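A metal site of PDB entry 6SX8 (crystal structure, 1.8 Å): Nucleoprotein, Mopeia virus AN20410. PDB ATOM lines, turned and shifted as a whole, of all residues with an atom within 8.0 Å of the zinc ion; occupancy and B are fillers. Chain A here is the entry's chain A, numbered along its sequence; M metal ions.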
ATOM      1  N   GLU A  28       7.319  21.771 -23.020  1.00  0.00           N
ATOM      2  CA  GLU A  28       7.366  21.207 -24.366  1.00  0.00           C
ATOM      3  C   GLU A  28       7.403  22.338 -25.382  1.00  0.00           C
ATOM      4  O   GLU A  28       6.801  23.393 -25.175  1.00  0.00           O
ATOM      5  CB  GLU A  28       6.170  20.310 -24.665  1.00  0.00           C
ATOM      6  CG  GLU A  28       5.885  19.204 -23.630  1.00  0.00           C
ATOM      7  CD  GLU A  28       7.105  18.358 -23.294  1.00  0.00           C
ATOM      8  OE1 GLU A  28       7.900  18.088 -24.222  1.00  0.00           O
ATOM      9  OE2 GLU A  28       7.263  17.940 -22.120  1.00  0.00           O
ATOM     10  N   VAL A  35       5.048  25.485 -26.136  1.00  0.00           N
ATOM     11  CA  VAL A  35       3.640  25.183 -26.324  1.00  0.00           C
ATOM     12  C   VAL A  35       2.994  24.567 -25.086  1.00  0.00           C
ATOM     13  O   VAL A  35       1.755  24.549 -25.019  1.00  0.00           O
ATOM     14  CB  VAL A  35       3.420  24.266 -27.545  1.00  0.00           C
ATOM     15  CG1 VAL A  35       3.777  25.011 -28.848  1.00  0.00           C
ATOM     16  CG2 VAL A  35       4.207  22.976 -27.400  1.00  0.00           C
ATOM     17  N   GLU A  36       3.754  24.060 -24.117  1.00  0.00           N
ATOM     18  CA  GLU A  36       3.164  23.538 -22.890  1.00  0.00           C
ATOM     19  C   GLU A  36       4.158  23.730 -21.750  1.00  0.00           C
ATOM     20  O   GLU A  36       5.348  23.486 -21.936  1.00  0.00           O
ATOM     21  CB  GLU A  36       2.793  22.058 -23.049  1.00  0.00           C
ATOM     22  CG  GLU A  36       1.875  21.525 -21.942  1.00  0.00           C
ATOM     23  CD  GLU A  36       1.759  20.014 -21.948  1.00  0.00           C
ATOM     24  OE1 GLU A  36       2.682  19.334 -22.447  1.00  0.00           O
ATOM     25  OE2 GLU A  36       0.736  19.514 -21.434  1.00  0.00           O
ATOM     26  N   ILE A  37       3.679  24.243 -20.606  1.00  0.00           N
ATOM     27  CA  ILE A  37       4.523  24.507 -19.436  1.00  0.00           C
ATOM     28  C   ILE A  37       3.861  23.921 -18.186  1.00  0.00           C
ATOM     29  O   ILE A  37       2.649  24.049 -17.999  1.00  0.00           O
ATOM     30  CB  ILE A  37       4.753  26.014 -19.240  1.00  0.00           C
ATOM     31  CG1 ILE A  37       5.487  26.609 -20.465  1.00  0.00           C
ATOM     32  CG2 ILE A  37       5.509  26.293 -17.941  1.00  0.00           C
ATOM     33  CD1 ILE A  37       5.847  28.070 -20.323  1.00  0.00           C
ATOM     34  N   ALA A  38       4.675  23.307 -17.328  1.00  0.00           N
ATOM     35  CA  ALA A  38       4.219  22.772 -16.048  1.00  0.00           C
ATOM     36  C   ALA A  38       5.193  23.150 -14.934  1.00  0.00           C
ATOM     37  O   ALA A  38       6.411  23.030 -15.112  1.00  0.00           O
ATOM     38  CB  ALA A  38       4.048  21.251 -16.123  1.00  0.00           C
ATOM     39  N   HIS A  49      -0.193  24.714 -14.804  1.00  0.00           N
ATOM     40  CA  HIS A  49      -0.123  23.991 -16.076  1.00  0.00           C
ATOM     41  C   HIS A  49      -0.968  24.691 -17.129  1.00  0.00           C
ATOM     42  O   HIS A  49      -2.170  24.909 -16.919  1.00  0.00           O
ATOM     43  CB  HIS A  49      -0.571  22.545 -15.887  1.00  0.00           C
ATOM     44  CG  HIS A  49      -0.575  21.744 -17.153  1.00  0.00           C
ATOM     45  ND1 HIS A  49      -1.563  20.829 -17.442  1.00  0.00           N
ATOM     46  CD2 HIS A  49       0.310  21.678 -18.172  1.00  0.00           C
ATOM     47  CE1 HIS A  49      -1.313  20.269 -18.615  1.00  0.00           C
ATOM     48  NE2 HIS A  49      -0.193  20.787 -19.088  1.00  0.00           N
ATOM     49  N   PHE A  50      -0.366  25.029 -18.258  1.00  0.00           N
ATOM     50  CA  PHE A  50      -1.072  25.826 -19.276  1.00  0.00           C
ATOM     51  C   PHE A  50      -0.393  25.597 -20.630  1.00  0.00           C
ATOM     52  O   PHE A  50       0.649  24.944 -20.719  1.00  0.00           O
ATOM     53  CB  PHE A  50      -1.095  27.301 -18.878  1.00  0.00           C
ATOM     54  CG  PHE A  50       0.276  27.919 -18.729  1.00  0.00           C
ATOM     55  CD1 PHE A  50       0.905  27.945 -17.500  1.00  0.00           C
ATOM     56  CD2 PHE A  50       0.916  28.470 -19.828  1.00  0.00           C
ATOM     57  CE1 PHE A  50       2.171  28.503 -17.358  1.00  0.00           C
ATOM     58  CE2 PHE A  50       2.182  29.028 -19.686  1.00  0.00           C
ATOM     59  CZ  PHE A  50       2.802  29.050 -18.458  1.00  0.00           C
ATOM     60  N   TYR A  51      -1.001  26.153 -21.680  1.00  0.00           N
ATOM     61  CA  TYR A  51      -0.545  25.901 -23.038  1.00  0.00           C
ATOM     62  C   TYR A  51      -0.315  27.212 -23.773  1.00  0.00           C
ATOM     63  O   TYR A  51      -0.690  28.293 -23.310  1.00  0.00           O
ATOM     64  CB  TYR A  51      -1.532  25.057 -23.824  1.00  0.00           C
ATOM     65  CG  TYR A  51      -2.077  23.903 -23.056  1.00  0.00           C
ATOM     66  CD1 TYR A  51      -1.413  22.694 -23.052  1.00  0.00           C
ATOM     67  CD2 TYR A  51      -3.241  24.034 -22.322  1.00  0.00           C
ATOM     68  CE1 TYR A  51      -1.903  21.624 -22.340  1.00  0.00           C
ATOM     69  CE2 TYR A  51      -3.755  22.967 -21.610  1.00  0.00           C
ATOM     70  CZ  TYR A  51      -3.072  21.769 -21.618  1.00  0.00           C
ATOM     71  OH  TYR A  51      -3.562  20.701 -20.920  1.00  0.00           O
ATOM     72  N   HIS A  68       5.417  15.516 -28.740  1.00  0.00           N
ATOM     73  CA  HIS A  68       4.280  15.791 -27.873  1.00  0.00           C
ATOM     74  C   HIS A  68       2.908  15.467 -28.473  1.00  0.00           C
ATOM     75  O   HIS A  68       1.934  15.412 -27.729  1.00  0.00           O
ATOM     76  CB  HIS A  68       4.302  17.269 -27.394  1.00  0.00           C
ATOM     77  CG  HIS A  68       4.350  18.282 -28.495  1.00  0.00           C
ATOM     78  ND1 HIS A  68       3.376  18.378 -29.470  1.00  0.00           N
ATOM     79  CD2 HIS A  68       5.224  19.281 -28.748  1.00  0.00           C
ATOM     80  CE1 HIS A  68       3.671  19.367 -30.288  1.00  0.00           C
ATOM     81  NE2 HIS A  68       4.786  19.941 -29.868  1.00  0.00           N
ATOM     82  N   ILE A  70       0.679  17.002 -30.047  1.00  0.00           N
ATOM     83  CA  ILE A  70      -0.379  17.996 -29.893  1.00  0.00           C
ATOM     84  C   ILE A  70      -0.862  18.418 -31.270  1.00  0.00           C
ATOM     85  O   ILE A  70      -0.050  18.704 -32.166  1.00  0.00           O
ATOM     86  CB  ILE A  70       0.119  19.196 -29.074  1.00  0.00           C
ATOM     87  CG1 ILE A  70       0.588  18.758 -27.693  1.00  0.00           C
ATOM     88  CG2 ILE A  70      -0.972  20.241 -28.941  1.00  0.00           C
ATOM     89  CD1 ILE A  70       1.294  19.861 -26.914  1.00  0.00           C
ATOM     90  N   TRP A 136       1.269   7.516 -16.645  1.00  0.00           N
ATOM     91  CA  TRP A 136       0.257   7.792 -17.662  1.00  0.00           C
ATOM     92  C   TRP A 136      -1.036   7.043 -17.342  1.00  0.00           C
ATOM     93  O   TRP A 136      -2.127   7.590 -17.546  1.00  0.00           O
ATOM     94  CB  TRP A 136       0.800   7.438 -19.056  1.00  0.00           C
ATOM     95  CG  TRP A 136       1.486   8.625 -19.735  1.00  0.00           C
ATOM     96  CD1 TRP A 136       2.776   9.050 -19.536  1.00  0.00           C
ATOM     97  CD2 TRP A 136       0.936   9.546 -20.690  1.00  0.00           C
ATOM     98  NE1 TRP A 136       3.065  10.156 -20.305  1.00  0.00           N
ATOM     99  CE2 TRP A 136       1.944  10.474 -21.031  1.00  0.00           C
ATOM    100  CE3 TRP A 136      -0.297   9.660 -21.332  1.00  0.00           C
ATOM    101  CZ2 TRP A 136       1.722  11.515 -21.948  1.00  0.00           C
ATOM    102  CZ3 TRP A 136      -0.510  10.700 -22.221  1.00  0.00           C
ATOM    103  CH2 TRP A 136       0.480  11.593 -22.547  1.00  0.00           C
ATOM    104  N   LYS A 140      -3.311  10.307 -16.853  1.00  0.00           N
ATOM    105  CA  LYS A 140      -3.685  10.686 -18.220  1.00  0.00           C
ATOM    106  C   LYS A 140      -4.812  11.709 -18.263  1.00  0.00           C
ATOM    107  O   LYS A 140      -4.775  12.633 -19.086  1.00  0.00           O
ATOM    108  CB  LYS A 140      -4.168   9.475 -19.025  1.00  0.00           C
ATOM    109  CG  LYS A 140      -3.303   9.047 -20.186  1.00  0.00           C
ATOM    110  CD  LYS A 140      -4.028   8.309 -21.370  1.00  0.00           C
ATOM    111  CE  LYS A 140      -3.141   8.385 -22.615  1.00  0.00           C
ATOM    112  NZ  LYS A 140      -3.693   7.958 -23.897  1.00  0.00           N
ATOM    113  N   LEU A 142      -5.471  14.156 -16.524  1.00  0.00           N
ATOM    114  CA  LEU A 142      -5.098  15.519 -16.177  1.00  0.00           C
ATOM    115  C   LEU A 142      -4.716  16.350 -17.385  1.00  0.00           C
ATOM    116  O   LEU A 142      -4.666  17.579 -17.265  1.00  0.00           O
ATOM    117  CB  LEU A 142      -3.946  15.532 -15.171  1.00  0.00           C
ATOM    118  CG  LEU A 142      -4.212  14.947 -13.779  1.00  0.00           C
ATOM    119  CD1 LEU A 142      -2.950  14.995 -12.900  1.00  0.00           C
ATOM    120  CD2 LEU A 142      -5.355  15.672 -13.100  1.00  0.00           C
ATOM    121  N   CYS A 143      -4.418  15.729 -18.525  1.00  0.00           N
ATOM    122  CA  CYS A 143      -4.058  16.469 -19.736  1.00  0.00           C
ATOM    123  C   CYS A 143      -4.410  15.612 -20.950  1.00  0.00           C
ATOM    124  O   CYS A 143      -3.764  14.594 -21.200  1.00  0.00           O
ATOM    125  CB  CYS A 143      -2.591  16.857 -19.754  1.00  0.00           C
ATOM    126  SG  CYS A 143      -2.145  17.770 -21.277  1.00  0.00           S
ATOM    127  N   ARG A 144      -5.414  16.043 -21.710  1.00  0.00           N
ATOM    128  CA  ARG A 144      -5.896  15.306 -22.879  1.00  0.00           C
ATOM    129  C   ARG A 144      -5.415  15.915 -24.195  1.00  0.00           C
ATOM    130  O   ARG A 144      -5.998  15.660 -25.247  1.00  0.00           O
ATOM    131  CB  ARG A 144      -7.428  15.237 -22.865  1.00  0.00           C
ATOM    132  CG  ARG A 144      -7.977  14.081 -22.048  1.00  0.00           C
ATOM    133  CD  ARG A 144      -9.292  13.569 -22.642  1.00  0.00           C
ATOM    134  NE  ARG A 144     -10.442  13.973 -21.824  1.00  0.00           N
ATOM    135  CZ  ARG A 144     -11.261  14.976 -22.128  1.00  0.00           C
ATOM    136  NH1 ARG A 144     -11.079  15.690 -23.234  1.00  0.00           N
ATOM    137  NH2 ARG A 144     -12.279  15.273 -21.325  1.00  0.00           N
ATOM    138  N   MET A 145      -4.349  16.699 -24.142  1.00  0.00           N
ATOM    139  CA  MET A 145      -3.937  17.501 -25.283  1.00  0.00           C
ATOM    140  C   MET A 145      -3.032  16.759 -26.253  1.00  0.00           C
ATOM    141  O   MET A 145      -2.721  17.290 -27.314  1.00  0.00           O
ATOM    142  CB  MET A 145      -3.247  18.765 -24.763  1.00  0.00           C
ATOM    143  CG  MET A 145      -4.204  19.671 -24.032  1.00  0.00           C
ATOM    144  SD  MET A 145      -5.265  20.525 -25.223  1.00  0.00           S
ATOM    145  CE  MET A 145      -4.024  21.112 -26.355  1.00  0.00           C
ATOM    146  N   HIS A 146      -2.614  15.539 -25.905  1.00  0.00           N
ATOM    147  CA  HIS A 146      -1.671  14.775 -26.720  1.00  0.00           C
ATOM    148  C   HIS A 146      -2.448  13.664 -27.424  1.00  0.00           C
ATOM    149  O   HIS A 146      -2.499  12.516 -26.992  1.00  0.00           O
ATOM    150  CB  HIS A 146      -0.546  14.272 -25.826  1.00  0.00           C
ATOM    151  CG  HIS A 146      -0.032  15.316 -24.876  1.00  0.00           C
ATOM    152  ND1 HIS A 146       1.073  16.100 -25.159  1.00  0.00           N
ATOM    153  CD2 HIS A 146      -0.461  15.707 -23.658  1.00  0.00           C
ATOM    154  CE1 HIS A 146       1.299  16.917 -24.149  1.00  0.00           C
ATOM    155  NE2 HIS A 146       0.367  16.711 -23.229  1.00  0.00           N
ATOM    156  N   PRO A 164       3.421   9.934 -25.811  1.00  0.00           N
ATOM    157  CA  PRO A 164       3.742  11.356 -26.050  1.00  0.00           C
ATOM    158  C   PRO A 164       4.313  12.005 -24.801  1.00  0.00           C
ATOM    159  O   PRO A 164       4.059  11.572 -23.677  1.00  0.00           O
ATOM    160  CB  PRO A 164       2.384  11.964 -26.431  1.00  0.00           C
ATOM    161  CG  PRO A 164       1.502  10.801 -26.781  1.00  0.00           C
ATOM    162  CD  PRO A 164       1.981   9.663 -25.944  1.00  0.00           C
ATOM    163  N   HIS A 165       5.094  13.048 -25.020  1.00  0.00           N
ATOM    164  CA  HIS A 165       5.720  13.808 -23.944  1.00  0.00           C
ATOM    165  C   HIS A 165       4.806  14.954 -23.536  1.00  0.00           C
ATOM    166  O   HIS A 165       4.437  15.795 -24.364  1.00  0.00           O
ATOM    167  CB  HIS A 165       7.087  14.341 -24.385  1.00  0.00           C
ATOM    168  CG  HIS A 165       8.120  13.266 -24.561  1.00  0.00           C
ATOM    169  ND1 HIS A 165       9.461  13.559 -24.736  1.00  0.00           N
ATOM    170  CD2 HIS A 165       8.018  11.916 -24.590  1.00  0.00           C
ATOM    171  CE1 HIS A 165      10.137  12.425 -24.862  1.00  0.00           C
ATOM    172  NE2 HIS A 165       9.284  11.422 -24.774  1.00  0.00           N
ATOM    173  N   CYS A 166       4.452  14.989 -22.249  1.00  0.00           N
ATOM    174  CA  CYS A 166       3.559  15.986 -21.687  1.00  0.00           C
ATOM    175  C   CYS A 166       4.305  16.695 -20.565  1.00  0.00           C
ATOM    176  O   CYS A 166       4.892  16.036 -19.685  1.00  0.00           O
ATOM    177  CB  CYS A 166       2.266  15.324 -21.158  1.00  0.00           C
ATOM    178  SG  CYS A 166       1.293  16.294 -19.971  1.00  0.00           S
ATOM    179  N   ALA A 167       4.306  18.033 -20.585  1.00  0.00           N
ATOM    180  CA  ALA A 167       5.052  18.794 -19.583  1.00  0.00           C
ATOM    181  C   ALA A 167       4.635  18.400 -18.164  1.00  0.00           C
ATOM    182  O   ALA A 167       5.487  18.209 -17.281  1.00  0.00           O
ATOM    183  CB  ALA A 167       4.861  20.297 -19.788  1.00  0.00           C
ATOM    184  N   LEU A 168       3.332  18.271 -17.952  1.00  0.00           N
ATOM    185  CA  LEU A 168       2.812  17.929 -16.634  1.00  0.00           C
ATOM    186  C   LEU A 168       3.242  16.531 -16.231  1.00  0.00           C
ATOM    187  O   LEU A 168       3.829  16.337 -15.156  1.00  0.00           O
ATOM    188  CB  LEU A 168       1.294  18.056 -16.601  1.00  0.00           C
ATOM    189  CG  LEU A 168       0.626  17.669 -15.266  1.00  0.00           C
ATOM    190  CD1 LEU A 168       1.161  18.534 -14.131  1.00  0.00           C
ATOM    191  CD2 LEU A 168      -0.890  17.806 -15.389  1.00  0.00           C
ATOM    192  N   LEU A 169       2.950  15.533 -17.066  1.00  0.00           N
ATOM    193  CA  LEU A 169       3.210  14.157 -16.636  1.00  0.00           C
ATOM    194  C   LEU A 169       4.699  13.877 -16.547  1.00  0.00           C
ATOM    195  O   LEU A 169       5.133  13.083 -15.709  1.00  0.00           O
ATOM    196  CB  LEU A 169       2.520  13.180 -17.601  1.00  0.00           C
ATOM    197  CG  LEU A 169       1.146  12.677 -17.120  1.00  0.00           C
ATOM    198  CD1 LEU A 169       0.230  13.816 -16.670  1.00  0.00           C
ATOM    199  CD2 LEU A 169       0.454  11.845 -18.203  1.00  0.00           C
ATOM    200  N   ASP A 170       5.508  14.564 -17.358  1.00  0.00           N
ATOM    201  CA  ASP A 170       6.956  14.470 -17.216  1.00  0.00           C
ATOM    202  C   ASP A 170       7.402  14.932 -15.838  1.00  0.00           C
ATOM    203  O   ASP A 170       8.291  14.316 -15.235  1.00  0.00           O
ATOM    204  CB  ASP A 170       7.652  15.295 -18.301  1.00  0.00           C
ATOM    205  CG  ASP A 170       7.692  14.608 -19.647  1.00  0.00           C
ATOM    206  OD1 ASP A 170       7.077  13.541 -19.807  1.00  0.00           O
ATOM    207  OD2 ASP A 170       8.344  15.136 -20.562  1.00  0.00           O
HETATM  208 ZN    ZN M   1       0.136  17.681 -21.503  1.00  0.00          ZN
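The zinc ion is bound by the side-chain carboxylate of Glu 36 (1.9 Å), a ring nitrogen (NE2) of His 146 (2.0 Å), the side-chain sulfur of Cys 143 (2.3 Å) and the side-chain sulfur of Cys 166 (2.4 Å). The zinc ion has four donor atoms within binding distance.
The side-chain carboxylate (OE2) of Glu 36 sits close to a ring nitrogen (NE2) of His 49, at 2.8 Å. OE1 of Glu 36 lies within hydrogen-bond range of N of Ala 167, at 2.8 Å. The backbone NH (N) of Glu 28 is in hydrogen-bond range of the backbone carbonyl oxygen (O) of Glu 36 (2.8 Å). A ring nitrogen (ND1) of His 146 lies close to the backbone carbonyl oxygen (O) of His 165 (3.5 Å). A ring nitrogen (ND1) of His 146 is in hydrogen-bond range of the backbone carbonyl oxygen of His 68, 2.8 Å away. The side-chain hydroxyl (OH) of Tyr 51 lies close to the side-chain sulfur (SG) of Cys 143 (3.3 Å). SG of Cys 143 sits close to N of Met 145. N of Leu 168 sits close to SG of Cys 166.
His 49 touches the zinc ion (NE2 to ZN, 3.9 Å). Within 4 Å of the zinc ion: Glu 36, His 49, Cys 143, His 146 and Cys 166.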
